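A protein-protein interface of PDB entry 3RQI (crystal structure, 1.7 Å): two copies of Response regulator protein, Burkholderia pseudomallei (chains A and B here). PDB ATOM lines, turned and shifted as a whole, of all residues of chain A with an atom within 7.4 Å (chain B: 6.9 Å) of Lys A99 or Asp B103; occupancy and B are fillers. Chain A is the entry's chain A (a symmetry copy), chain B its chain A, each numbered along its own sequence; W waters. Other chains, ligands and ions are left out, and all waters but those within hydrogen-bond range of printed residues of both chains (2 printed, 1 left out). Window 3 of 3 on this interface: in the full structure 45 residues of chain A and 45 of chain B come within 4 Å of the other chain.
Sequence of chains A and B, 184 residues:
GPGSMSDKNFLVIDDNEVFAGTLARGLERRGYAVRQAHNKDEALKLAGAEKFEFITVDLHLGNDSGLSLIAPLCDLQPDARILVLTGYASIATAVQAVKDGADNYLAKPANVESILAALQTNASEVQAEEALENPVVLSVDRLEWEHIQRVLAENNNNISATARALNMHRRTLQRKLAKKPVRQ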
ATOM      1  N   ILE A  70     -12.772 -26.362   5.845  1.00  0.00           N
ATOM      2  CA  ILE A  70     -13.740 -25.382   5.338  1.00  0.00           C
ATOM      3  C   ILE A  70     -15.201 -25.895   5.396  1.00  0.00           C
ATOM      4  O   ILE A  70     -16.093 -25.185   5.890  1.00  0.00           O
ATOM      5  CB  ILE A  70     -13.367 -24.958   3.929  1.00  0.00           C
ATOM      6  CG1 ILE A  70     -12.024 -24.220   3.969  1.00  0.00           C
ATOM      7  CG2 ILE A  70     -14.484 -24.046   3.366  1.00  0.00           C
ATOM      8  CD1 ILE A  70     -11.364 -24.021   2.580  1.00  0.00           C
ATOM      9  N   ALA A  71     -15.452 -27.103   4.887  1.00  0.00           N
ATOM     10  CA  ALA A  71     -16.807 -27.668   4.967  1.00  0.00           C
ATOM     11  C   ALA A  71     -17.358 -27.783   6.411  1.00  0.00           C
ATOM     12  O   ALA A  71     -18.489 -27.348   6.657  1.00  0.00           O
ATOM     13  CB  ALA A  71     -16.898 -29.038   4.206  1.00  0.00           C
ATOM     14  N   THR A  93      -6.030 -24.928  -5.347  1.00  0.00           N
ATOM     15  CA  THR A  93      -6.607 -24.853  -3.992  1.00  0.00           C
ATOM     16  C   THR A  93      -7.734 -23.837  -3.880  1.00  0.00           C
ATOM     17  O   THR A  93      -8.640 -24.011  -3.064  1.00  0.00           O
ATOM     18  CB  THR A  93      -5.536 -24.606  -2.947  1.00  0.00           C
ATOM     19  OG1 THR A  93      -4.797 -23.434  -3.293  1.00  0.00           O
ATOM     20  CG2 THR A  93      -4.626 -25.783  -2.860  1.00  0.00           C
ATOM     21  N   ALA A  94      -7.695 -22.789  -4.704  1.00  0.00           N
ATOM     22  CA  ALA A  94      -8.769 -21.783  -4.691  1.00  0.00           C
ATOM     23  C   ALA A  94     -10.068 -22.413  -5.222  1.00  0.00           C
ATOM     24  O   ALA A  94     -11.101 -22.265  -4.617  1.00  0.00           O
ATOM     25  CB  ALA A  94      -8.338 -20.561  -5.507  1.00  0.00           C
ATOM     26  N   VAL A  95      -9.979 -23.152  -6.333  1.00  0.00           N
ATOM     27  CA  VAL A  95     -11.141 -23.893  -6.873  1.00  0.00           C
ATOM     28  C   VAL A  95     -11.723 -24.786  -5.762  1.00  0.00           C
ATOM     29  O   VAL A  95     -12.939 -24.691  -5.507  1.00  0.00           O
ATOM     30  CB  VAL A  95     -10.718 -24.740  -8.118  1.00  0.00           C
ATOM     31  CG1 VAL A  95     -11.822 -25.736  -8.522  1.00  0.00           C
ATOM     32  CG2 VAL A  95     -10.362 -23.838  -9.323  1.00  0.00           C
ATOM     33  N   GLN A  96     -10.906 -25.640  -5.104  1.00  0.00           N
ATOM     34  CA  GLN A  96     -11.456 -26.570  -4.132  1.00  0.00           C
ATOM     35  C   GLN A  96     -11.990 -25.843  -2.895  1.00  0.00           C
ATOM     36  O   GLN A  96     -13.031 -26.229  -2.353  1.00  0.00           O
ATOM     37  CB  GLN A  96     -10.432 -27.641  -3.756  1.00  0.00           C
ATOM     38  CG  GLN A  96     -11.036 -28.815  -2.955  1.00  0.00           C
ATOM     39  CD  GLN A  96     -12.127 -29.496  -3.775  1.00  0.00           C
ATOM     40  OE1 GLN A  96     -11.936 -29.767  -4.966  1.00  0.00           O
ATOM     41  NE2 GLN A  96     -13.277 -29.751  -3.151  1.00  0.00           N
ATOM     42  N   ALA A  97     -11.291 -24.793  -2.469  1.00  0.00           N
ATOM     43  CA  ALA A  97     -11.765 -24.040  -1.306  1.00  0.00           C
ATOM     44  C   ALA A  97     -13.159 -23.462  -1.496  1.00  0.00           C
ATOM     45  O   ALA A  97     -14.009 -23.491  -0.565  1.00  0.00           O
ATOM     46  CB  ALA A  97     -10.786 -22.919  -0.943  1.00  0.00           C
ATOM     47  N   VAL A  98     -13.415 -22.972  -2.703  1.00  0.00           N
ATOM     48  CA  VAL A  98     -14.731 -22.385  -2.986  1.00  0.00           C
ATOM     49  C   VAL A  98     -15.762 -23.497  -3.049  1.00  0.00           C
ATOM     50  O   VAL A  98     -16.887 -23.357  -2.544  1.00  0.00           O
ATOM     51  CB  VAL A  98     -14.708 -21.523  -4.285  1.00  0.00           C
ATOM     52  CG1 VAL A  98     -16.150 -21.071  -4.653  1.00  0.00           C
ATOM     53  CG2 VAL A  98     -13.729 -20.385  -4.140  1.00  0.00           C
ATOM     54  N   LYS A  99     -15.404 -24.651  -3.630  1.00  0.00           N
ATOM     55  CA  LYS A  99     -16.366 -25.758  -3.651  1.00  0.00           C
ATOM     56  C   LYS A  99     -16.768 -26.194  -2.237  1.00  0.00           C
ATOM     57  O   LYS A  99     -17.916 -26.579  -1.988  1.00  0.00           O
ATOM     58  CB  LYS A  99     -15.784 -26.974  -4.401  1.00  0.00           C
ATOM     59  CG  LYS A  99     -15.604 -26.809  -5.892  1.00  0.00           C
ATOM     60  CD  LYS A  99     -15.289 -28.178  -6.489  1.00  0.00           C
ATOM     61  CE  LYS A  99     -15.074 -28.082  -7.979  1.00  0.00           C
ATOM     62  NZ  LYS A  99     -14.955 -29.421  -8.586  1.00  0.00           N
ATOM     63  N   ASP A 100     -15.803 -26.117  -1.312  1.00  0.00           N
ATOM     64  CA  ASP A 100     -15.955 -26.540   0.084  1.00  0.00           C
ATOM     65  C   ASP A 100     -16.789 -25.542   0.898  1.00  0.00           C
ATOM     66  O   ASP A 100     -17.248 -25.869   2.016  1.00  0.00           O
ATOM     67  CB  ASP A 100     -14.562 -26.694   0.744  1.00  0.00           C
ATOM     68  CG  ASP A 100     -13.769 -27.886   0.218  1.00  0.00           C
ATOM     69  OD1 ASP A 100     -14.324 -28.738  -0.492  1.00  0.00           O
ATOM     70  OD2 ASP A 100     -12.551 -27.933   0.504  1.00  0.00           O
ATOM     71  N   GLY A 101     -16.972 -24.345   0.333  1.00  0.00           N
ATOM     72  CA  GLY A 101     -17.787 -23.305   0.943  1.00  0.00           C
ATOM     73  C   GLY A 101     -17.134 -21.980   1.268  1.00  0.00           C
ATOM     74  O   GLY A 101     -17.828 -21.089   1.788  1.00  0.00           O
ATOM     75  N   ALA A 102     -15.841 -21.845   0.975  1.00  0.00           N
ATOM     76  CA  ALA A 102     -15.184 -20.558   1.233  1.00  0.00           C
ATOM     77  C   ALA A 102     -15.827 -19.454   0.402  1.00  0.00           C
ATOM     78  O   ALA A 102     -16.156 -19.636  -0.783  1.00  0.00           O
ATOM     79  CB  ALA A 102     -13.708 -20.609   0.961  1.00  0.00           C
ATOM     80  N   ILE B  70     -21.291 -18.734 -17.421  1.00  0.00           N
ATOM     81  CA  ILE B  70     -21.251 -19.991 -16.663  1.00  0.00           C
ATOM     82  C   ILE B  70     -22.597 -20.318 -15.969  1.00  0.00           C
ATOM     83  O   ILE B  70     -23.103 -21.446 -16.089  1.00  0.00           O
ATOM     84  CB  ILE B  70     -20.113 -19.963 -15.660  1.00  0.00           C
ATOM     85  CG1 ILE B  70     -18.781 -19.900 -16.417  1.00  0.00           C
ATOM     86  CG2 ILE B  70     -20.189 -21.232 -14.777  1.00  0.00           C
ATOM     87  CD1 ILE B  70     -17.560 -19.537 -15.532  1.00  0.00           C
ATOM     88  N   CYS B  74     -25.040 -23.531 -16.742  1.00  0.00           N
ATOM     89  CA  CYS B  74     -25.446 -24.506 -15.751  1.00  0.00           C
ATOM     90  C   CYS B  74     -26.965 -24.670 -15.747  1.00  0.00           C
ATOM     91  O   CYS B  74     -27.450 -25.776 -15.520  1.00  0.00           O
ATOM     92  CB  CYS B  74     -24.985 -24.082 -14.364  1.00  0.00           C
ATOM     93  SG  CYS B  74     -23.240 -24.160 -14.138  1.00  0.00           S
ATOM     94  N   ASP B  79     -26.725 -31.256 -16.222  1.00  0.00           N
ATOM     95  CA  ASP B  79     -25.937 -32.491 -16.189  1.00  0.00           C
ATOM     96  C   ASP B  79     -24.469 -32.334 -16.693  1.00  0.00           C
ATOM     97  O   ASP B  79     -23.625 -33.165 -16.374  1.00  0.00           O
ATOM     98  CB  ASP B  79     -26.640 -33.658 -16.926  1.00  0.00           C
ATOM     99  CG  ASP B  79     -27.948 -34.127 -16.245  1.00  0.00           C
ATOM    100  OD1 ASP B  79     -28.033 -34.136 -14.996  1.00  0.00           O
ATOM    101  OD2 ASP B  79     -28.890 -34.518 -16.977  1.00  0.00           O
ATOM    102  N   ALA B  80     -24.172 -31.273 -17.430  1.00  0.00           N
ATOM    103  CA  ALA B  80     -22.830 -31.086 -18.048  1.00  0.00           C
ATOM    104  C   ALA B  80     -21.710 -30.847 -17.035  1.00  0.00           C
ATOM    105  O   ALA B  80     -21.935 -30.211 -16.000  1.00  0.00           O
ATOM    106  CB  ALA B  80     -22.882 -29.899 -19.019  1.00  0.00           C
ATOM    107  N   ARG B  81     -20.515 -31.380 -17.336  1.00  0.00           N
ATOM    108  CA  ARG B  81     -19.274 -30.970 -16.637  1.00  0.00           C
ATOM    109  C   ARG B  81     -18.747 -29.748 -17.365  1.00  0.00           C
ATOM    110  O   ARG B  81     -18.672 -29.744 -18.577  1.00  0.00           O
ATOM    111  CB  ARG B  81     -18.231 -32.092 -16.677  1.00  0.00           C
ATOM    112  CG  ARG B  81     -18.683 -33.482 -16.253  1.00  0.00           C
ATOM    113  CD  ARG B  81     -18.755 -33.732 -14.775  1.00  0.00           C
ATOM    114  NE  ARG B  81     -17.576 -33.293 -14.000  1.00  0.00           N
ATOM    115  CZ  ARG B  81     -17.606 -33.109 -12.685  1.00  0.00           C
ATOM    116  NH1 ARG B  81     -18.729 -33.327 -11.995  1.00  0.00           N
ATOM    117  NH2 ARG B  81     -16.526 -32.687 -12.042  1.00  0.00           N
ATOM    118  N   ILE B  82     -18.418 -28.687 -16.631  1.00  0.00           N
ATOM    119  CA  ILE B  82     -18.064 -27.424 -17.242  1.00  0.00           C
ATOM    120  C   ILE B  82     -16.676 -27.012 -16.757  1.00  0.00           C
ATOM    121  O   ILE B  82     -16.410 -26.943 -15.547  1.00  0.00           O
ATOM    122  CB  ILE B  82     -19.135 -26.335 -16.880  1.00  0.00           C
ATOM    123  CG1 ILE B  82     -20.499 -26.698 -17.536  1.00  0.00           C
ATOM    124  CG2 ILE B  82     -18.666 -24.970 -17.346  1.00  0.00           C
ATOM    125  CD1 ILE B  82     -21.620 -25.753 -17.138  1.00  0.00           C
ATOM    126  N   LEU B  83     -15.770 -26.736 -17.701  1.00  0.00           N
ATOM    127  CA  LEU B  83     -14.372 -26.420 -17.370  1.00  0.00           C
ATOM    128  C   LEU B  83     -14.061 -25.043 -17.970  1.00  0.00           C
ATOM    129  O   LEU B  83     -14.269 -24.813 -19.176  1.00  0.00           O
ATOM    130  CB  LEU B  83     -13.449 -27.471 -18.030  1.00  0.00           C
ATOM    131  CG  LEU B  83     -11.954 -27.143 -18.077  1.00  0.00           C
ATOM    132  CD1 LEU B  83     -11.306 -27.227 -16.640  1.00  0.00           C
ATOM    133  CD2 LEU B  83     -11.229 -28.091 -19.076  1.00  0.00           C
ATOM    134  N   VAL B  84     -13.559 -24.136 -17.157  1.00  0.00           N
ATOM    135  CA  VAL B  84     -12.971 -22.876 -17.695  1.00  0.00           C
ATOM    136  C   VAL B  84     -11.595 -23.203 -18.222  1.00  0.00           C
ATOM    137  O   VAL B  84     -10.774 -23.878 -17.554  1.00  0.00           O
ATOM    138  CB  VAL B  84     -12.857 -21.745 -16.632  1.00  0.00           C
ATOM    139  CG1 VAL B  84     -12.000 -20.546 -17.183  1.00  0.00           C
ATOM    140  CG2 VAL B  84     -14.262 -21.268 -16.203  1.00  0.00           C
ATOM    141  N   ALA B  97     -15.574 -18.149 -11.035  1.00  0.00           N
ATOM    142  CA  ALA B  97     -16.067 -19.191 -11.939  1.00  0.00           C
ATOM    143  C   ALA B  97     -16.687 -20.372 -11.209  1.00  0.00           C
ATOM    144  O   ALA B  97     -17.746 -20.915 -11.629  1.00  0.00           O
ATOM    145  CB  ALA B  97     -14.949 -19.685 -12.864  1.00  0.00           C
ATOM    146  N   VAL B  98     -16.063 -20.752 -10.101  1.00  0.00           N
ATOM    147  CA  VAL B  98     -16.580 -21.887  -9.326  1.00  0.00           C
ATOM    148  C   VAL B  98     -17.867 -21.469  -8.642  1.00  0.00           C
ATOM    149  O   VAL B  98     -18.842 -22.237  -8.585  1.00  0.00           O
ATOM    150  CB  VAL B  98     -15.520 -22.425  -8.318  1.00  0.00           C
ATOM    151  CG1 VAL B  98     -16.157 -23.499  -7.392  1.00  0.00           C
ATOM    152  CG2 VAL B  98     -14.293 -22.903  -9.053  1.00  0.00           C
ATOM    153  N   LYS B  99     -17.936 -20.228  -8.138  1.00  0.00           N
ATOM    154  CA  LYS B  99     -19.191 -19.785  -7.524  1.00  0.00           C
ATOM    155  C   LYS B  99     -20.359 -19.818  -8.516  1.00  0.00           C
ATOM    156  O   LYS B  99     -21.501 -20.119  -8.152  1.00  0.00           O
ATOM    157  CB  LYS B  99     -19.051 -18.352  -6.966  1.00  0.00           C
ATOM    158  CG  LYS B  99     -18.148 -18.193  -5.766  1.00  0.00           C
ATOM    159  CD  LYS B  99     -18.351 -16.791  -5.198  1.00  0.00           C
ATOM    160  CE  LYS B  99     -17.458 -16.556  -4.006  1.00  0.00           C
ATOM    161  NZ  LYS B  99     -17.782 -15.277  -3.344  1.00  0.00           N
ATOM    162  N   GLY B 101     -20.739 -21.842 -10.930  1.00  0.00           N
ATOM    163  CA  GLY B 101     -21.074 -23.226 -11.232  1.00  0.00           C
ATOM    164  C   GLY B 101     -20.070 -24.055 -12.000  1.00  0.00           C
ATOM    165  O   GLY B 101     -20.351 -25.238 -12.259  1.00  0.00           O
ATOM    166  N   ALA B 102     -18.932 -23.463 -12.359  1.00  0.00           N
ATOM    167  CA  ALA B 102     -17.913 -24.249 -13.067  1.00  0.00           C
ATOM    168  C   ALA B 102     -17.424 -25.399 -12.194  1.00  0.00           C
ATOM    169  O   ALA B 102     -17.209 -25.251 -10.979  1.00  0.00           O
ATOM    170  CB  ALA B 102     -16.747 -23.407 -13.502  1.00  0.00           C
ATOM    171  N   ASP B 103     -17.200 -26.538 -12.831  1.00  0.00           N
ATOM    172  CA  ASP B 103     -16.645 -27.679 -12.125  1.00  0.00           C
ATOM    173  C   ASP B 103     -15.121 -27.636 -11.947  1.00  0.00           C
ATOM    174  O   ASP B 103     -14.597 -28.246 -11.020  1.00  0.00           O
ATOM    175  CB  ASP B 103     -17.062 -29.007 -12.802  1.00  0.00           C
ATOM    176  CG  ASP B 103     -18.548 -29.181 -12.840  1.00  0.00           C
ATOM    177  OD1 ASP B 103     -19.140 -29.412 -11.755  1.00  0.00           O
ATOM    178  OD2 ASP B 103     -19.133 -29.050 -13.924  1.00  0.00           O
ATOM    179  N   ASN B 104     -14.401 -26.955 -12.849  1.00  0.00           N
ATOM    180  CA  ASN B 104     -12.950 -26.889 -12.732  1.00  0.00           C
ATOM    181  C   ASN B 104     -12.415 -25.757 -13.586  1.00  0.00           C
ATOM    182  O   ASN B 104     -13.182 -25.067 -14.294  1.00  0.00           O
ATOM    183  CB  ASN B 104     -12.298 -28.234 -13.146  1.00  0.00           C
ATOM    184  CG  ASN B 104     -11.003 -28.501 -12.429  1.00  0.00           C
ATOM    185  OD1 ASN B 104     -10.476 -27.637 -11.687  1.00  0.00           O
ATOM    186  ND2 ASN B 104     -10.458 -29.708 -12.643  1.00  0.00           N
ATOM    187  N   TYR B 105     -11.100 -25.554 -13.533  1.00  0.00           N
ATOM    188  CA  TYR B 105     -10.524 -24.376 -14.184  1.00  0.00           C
ATOM    189  C   TYR B 105      -9.106 -24.749 -14.536  1.00  0.00           C
ATOM    190  O   TYR B 105      -8.382 -25.293 -13.703  1.00  0.00           O
ATOM    191  CB  TYR B 105     -10.583 -23.213 -13.183  1.00  0.00           C
ATOM    192  CG  TYR B 105     -10.054 -21.829 -13.596  1.00  0.00           C
ATOM    193  CD1 TYR B 105     -10.936 -20.743 -13.671  1.00  0.00           C
ATOM    194  CD2 TYR B 105      -8.676 -21.619 -13.862  1.00  0.00           C
ATOM    195  CE1 TYR B 105     -10.482 -19.455 -13.972  1.00  0.00           C
ATOM    196  CE2 TYR B 105      -8.206 -20.349 -14.179  1.00  0.00           C
ATOM    197  CZ  TYR B 105      -9.112 -19.276 -14.218  1.00  0.00           C
ATOM    198  OH  TYR B 105      -8.652 -18.033 -14.518  1.00  0.00           O
ATOM    199  N   ALA B 118      -9.330 -33.000 -16.354  1.00  0.00           N
ATOM    200  CA  ALA B 118      -9.844 -31.872 -15.544  1.00  0.00           C
ATOM    201  C   ALA B 118     -11.372 -31.863 -15.488  1.00  0.00           C
ATOM    202  O   ALA B 118     -11.985 -31.315 -14.558  1.00  0.00           O
ATOM    203  CB  ALA B 118      -9.331 -30.589 -16.082  1.00  0.00           C
ATOM    204  N   LEU B 119     -11.990 -32.507 -16.469  1.00  0.00           N
ATOM    205  CA  LEU B 119     -13.451 -32.638 -16.488  1.00  0.00           C
ATOM    206  C   LEU B 119     -14.055 -33.750 -15.657  1.00  0.00           C
ATOM    207  O   LEU B 119     -15.283 -33.831 -15.533  1.00  0.00           O
ATOM    208  CB  LEU B 119     -13.923 -32.789 -17.937  1.00  0.00           C
ATOM    209  CG  LEU B 119     -13.926 -31.478 -18.701  1.00  0.00           C
ATOM    210  CD1 LEU B 119     -13.830 -31.731 -20.233  1.00  0.00           C
ATOM    211  CD2 LEU B 119     -15.190 -30.629 -18.368  1.00  0.00           C
ATOM    212  N   GLN B 120     -13.228 -34.673 -15.127  1.00  0.00           N
ATOM    213  CA  GLN B 120     -13.736 -35.828 -14.417  1.00  0.00           C
ATOM    214  C   GLN B 120     -14.138 -35.494 -12.993  1.00  0.00           C
ATOM    215  O   GLN B 120     -13.599 -34.566 -12.395  1.00  0.00           O
ATOM    216  CB  GLN B 120     -12.652 -36.919 -14.350  1.00  0.00           C
ATOM    217  CG  GLN B 120     -12.114 -37.274 -15.727  1.00  0.00           C
ATOM    218  CD  GLN B 120     -13.202 -37.810 -16.626  1.00  0.00           C
ATOM    219  OE1 GLN B 120     -13.849 -38.800 -16.280  1.00  0.00           O
ATOM    220  NE2 GLN B 120     -13.414 -37.168 -17.781  1.00  0.00           N
ATOM    221  N   ASN B 122     -14.237 -35.323  -9.130  1.00  0.00           N
ATOM    222  CA  ASN B 122     -13.182 -35.266  -8.101  1.00  0.00           C
ATOM    223  C   ASN B 122     -11.832 -34.729  -8.613  1.00  0.00           C
ATOM    224  O   ASN B 122     -10.862 -34.718  -7.849  1.00  0.00           O
ATOM    225  CB  ASN B 122     -12.962 -36.617  -7.419  1.00  0.00           C
ATOM    226  CG  ASN B 122     -14.212 -37.137  -6.689  1.00  0.00           C
ATOM    227  OD1 ASN B 122     -14.794 -36.436  -5.838  1.00  0.00           O
ATOM    228  ND2 ASN B 122     -14.604 -38.390  -6.991  1.00  0.00           N
ATOM    229  N   ALA B 123     -11.776 -34.281  -9.867  1.00  0.00           N
ATOM    230  CA  ALA B 123     -10.473 -33.820 -10.408  1.00  0.00           C
ATOM    231  C   ALA B 123      -9.889 -32.672  -9.615  1.00  0.00           C
ATOM    232  O   ALA B 123      -8.683 -32.682  -9.276  1.00  0.00           O
ATOM    233  CB  ALA B 123     -10.585 -33.462 -11.896  1.00  0.00           C
ATOM    234  N   SER B 124     -10.748 -31.715  -9.252  1.00  0.00           N
ATOM    235  CA  SER B 124     -10.308 -30.569  -8.448  1.00  0.00           C
ATOM    236  C   SER B 124      -9.703 -30.972  -7.106  1.00  0.00           C
ATOM    237  O   SER B 124      -8.692 -30.397  -6.694  1.00  0.00           O
ATOM    238  CB  SER B 124     -11.425 -29.489  -8.264  1.00  0.00           C
ATOM    239  OG  SER B 124     -12.559 -30.023  -7.564  1.00  0.00           O
ATOM    240  N   GLU B 125     -10.325 -31.940  -6.426  1.00  0.00           N
ATOM    241  CA  GLU B 125      -9.801 -32.360  -5.119  1.00  0.00           C
ATOM    242  C   GLU B 125      -8.403 -32.949  -5.274  1.00  0.00           C
ATOM    243  O   GLU B 125      -7.528 -32.616  -4.475  1.00  0.00           O
ATOM    244  CB  GLU B 125     -10.750 -33.323  -4.384  1.00  0.00           C
ATOM    245  CG  GLU B 125     -10.310 -33.764  -2.956  1.00  0.00           C
ATOM    246  CD  GLU B 125      -9.801 -32.637  -2.076  1.00  0.00           C
ATOM    247  OE1 GLU B 125      -8.580 -32.608  -1.781  1.00  0.00           O
ATOM    248  OE2 GLU B 125     -10.613 -31.778  -1.673  1.00  0.00           O
HETATM  249  O   HOH W   1     -17.997 -29.623  -9.554  1.00  0.00           O
HETATM  250  O   HOH W   2     -11.376 -30.139   0.175  1.00  0.00           O
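The side-chain amide oxygen of Gln A96 lies within hydrogen-bond range of the backbone NH of Glu B125 (3.1 Å).
The side-chain hydroxyl (OG) of Ser B124 lies within hydrogen-bond range of the side-chain amide oxygen (OE1) of Gln A96 (2.7 Å).
O of Asp B103 lies within hydrogen-bond range of NZ of Lys A99 (2.7 Å).
NZ of Lys A99 is in hydrogen-bond range of OG of Ser B124, at 2.7 Å.
O of Ile B82 sits at hydrogen-bond distance from N of Asn B104.
ND2 of Asn B104 is in hydrogen-bond range of O of Ala B118 (2.9 Å).
The backbone NH (N) of Ile B82 lies within hydrogen-bond range of the side-chain carboxylate (OD2) of Asp B103, at 2.8 Å.
The side-chain carboxylate (OD1) of Asp B103 is in salt-bridge range of the guanidinium group (NH1) of Arg B81 (3.9 Å).
The side-chain amide nitrogen of Gln A96 is in hydrogen-bond range of the side-chain carboxylate of Asp A100, at 3.0 Å.
O of Asn B104 sits at hydrogen-bond distance from N of Val B84, at 3.0 Å.
Val A95 touches Val B98 (CG1 to CG2, 3.8 Å).
Val A95 touches Asn B104 (CG1 to OD1, 3.9 Å).
Tyr B105 touches Val A95.
CG1 of Val A95 touches CB of Ser B124, at 3.8 Å.
Val A98 touches Val B98 (CG1 to CG1, 3.7 Å).
Lys B99 touches Val A98.
Lys A99 touches Val B98.
Printed residues of chain B within 4 Å of Val A95: Val B98, Asn B104, Tyr B105 and Ser B124.
Val B84 touches none of the printed residues of chain A.
Of the printed residues of chain A, Lys B99 touches Val A98.
Of the printed residues of chain A, Glu B125 touches Gln A96.
The nearest printed residue of chain B that does not touch Lys A99 is Ala B102 (4.6 Å).
The nearest residue of chain A that does not touch Asp B103 is Val A95 (4.5 Å).
The nearest printed residue of chain A that does not touch Asn B104 is Lys A99 (5.0 Å).
Printed residues of chain B that touch a printed residue of chain A: Val B98, Lys B99, Asp B103, Asn B104, Tyr B105, Ser B124 and Glu B125.
Hydrophobic or aromatic side chains of chain B within 4 Å of the printed part of chain A: Val B98 and Tyr B105.
Of the 12 printed residues of chain A, 4 touch a printed residue of chain B.
Hydrophobic or aromatic side chains of chain A within 4 Å of the printed part of chain B: Val A95 and Val A98.
Among the printed residues, 11 pairs touch across the chains.
Among the printed residues, no Asp or Glu carboxylate lies within 4 Å of a Lys or Arg side-chain nitrogen of the other chain.
Val A98 touches its own counterpart, Val B98.
Val A98 touches Lys B99, and with the chains exchanged Lys A99 touches Val B98.
Water W1 bridges the side-chain carboxylate of Asp B103 and the side-chain amino group of Lys A99.
Water W2 bridges OD2 of Asp A100 and OE2 of Glu B125.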
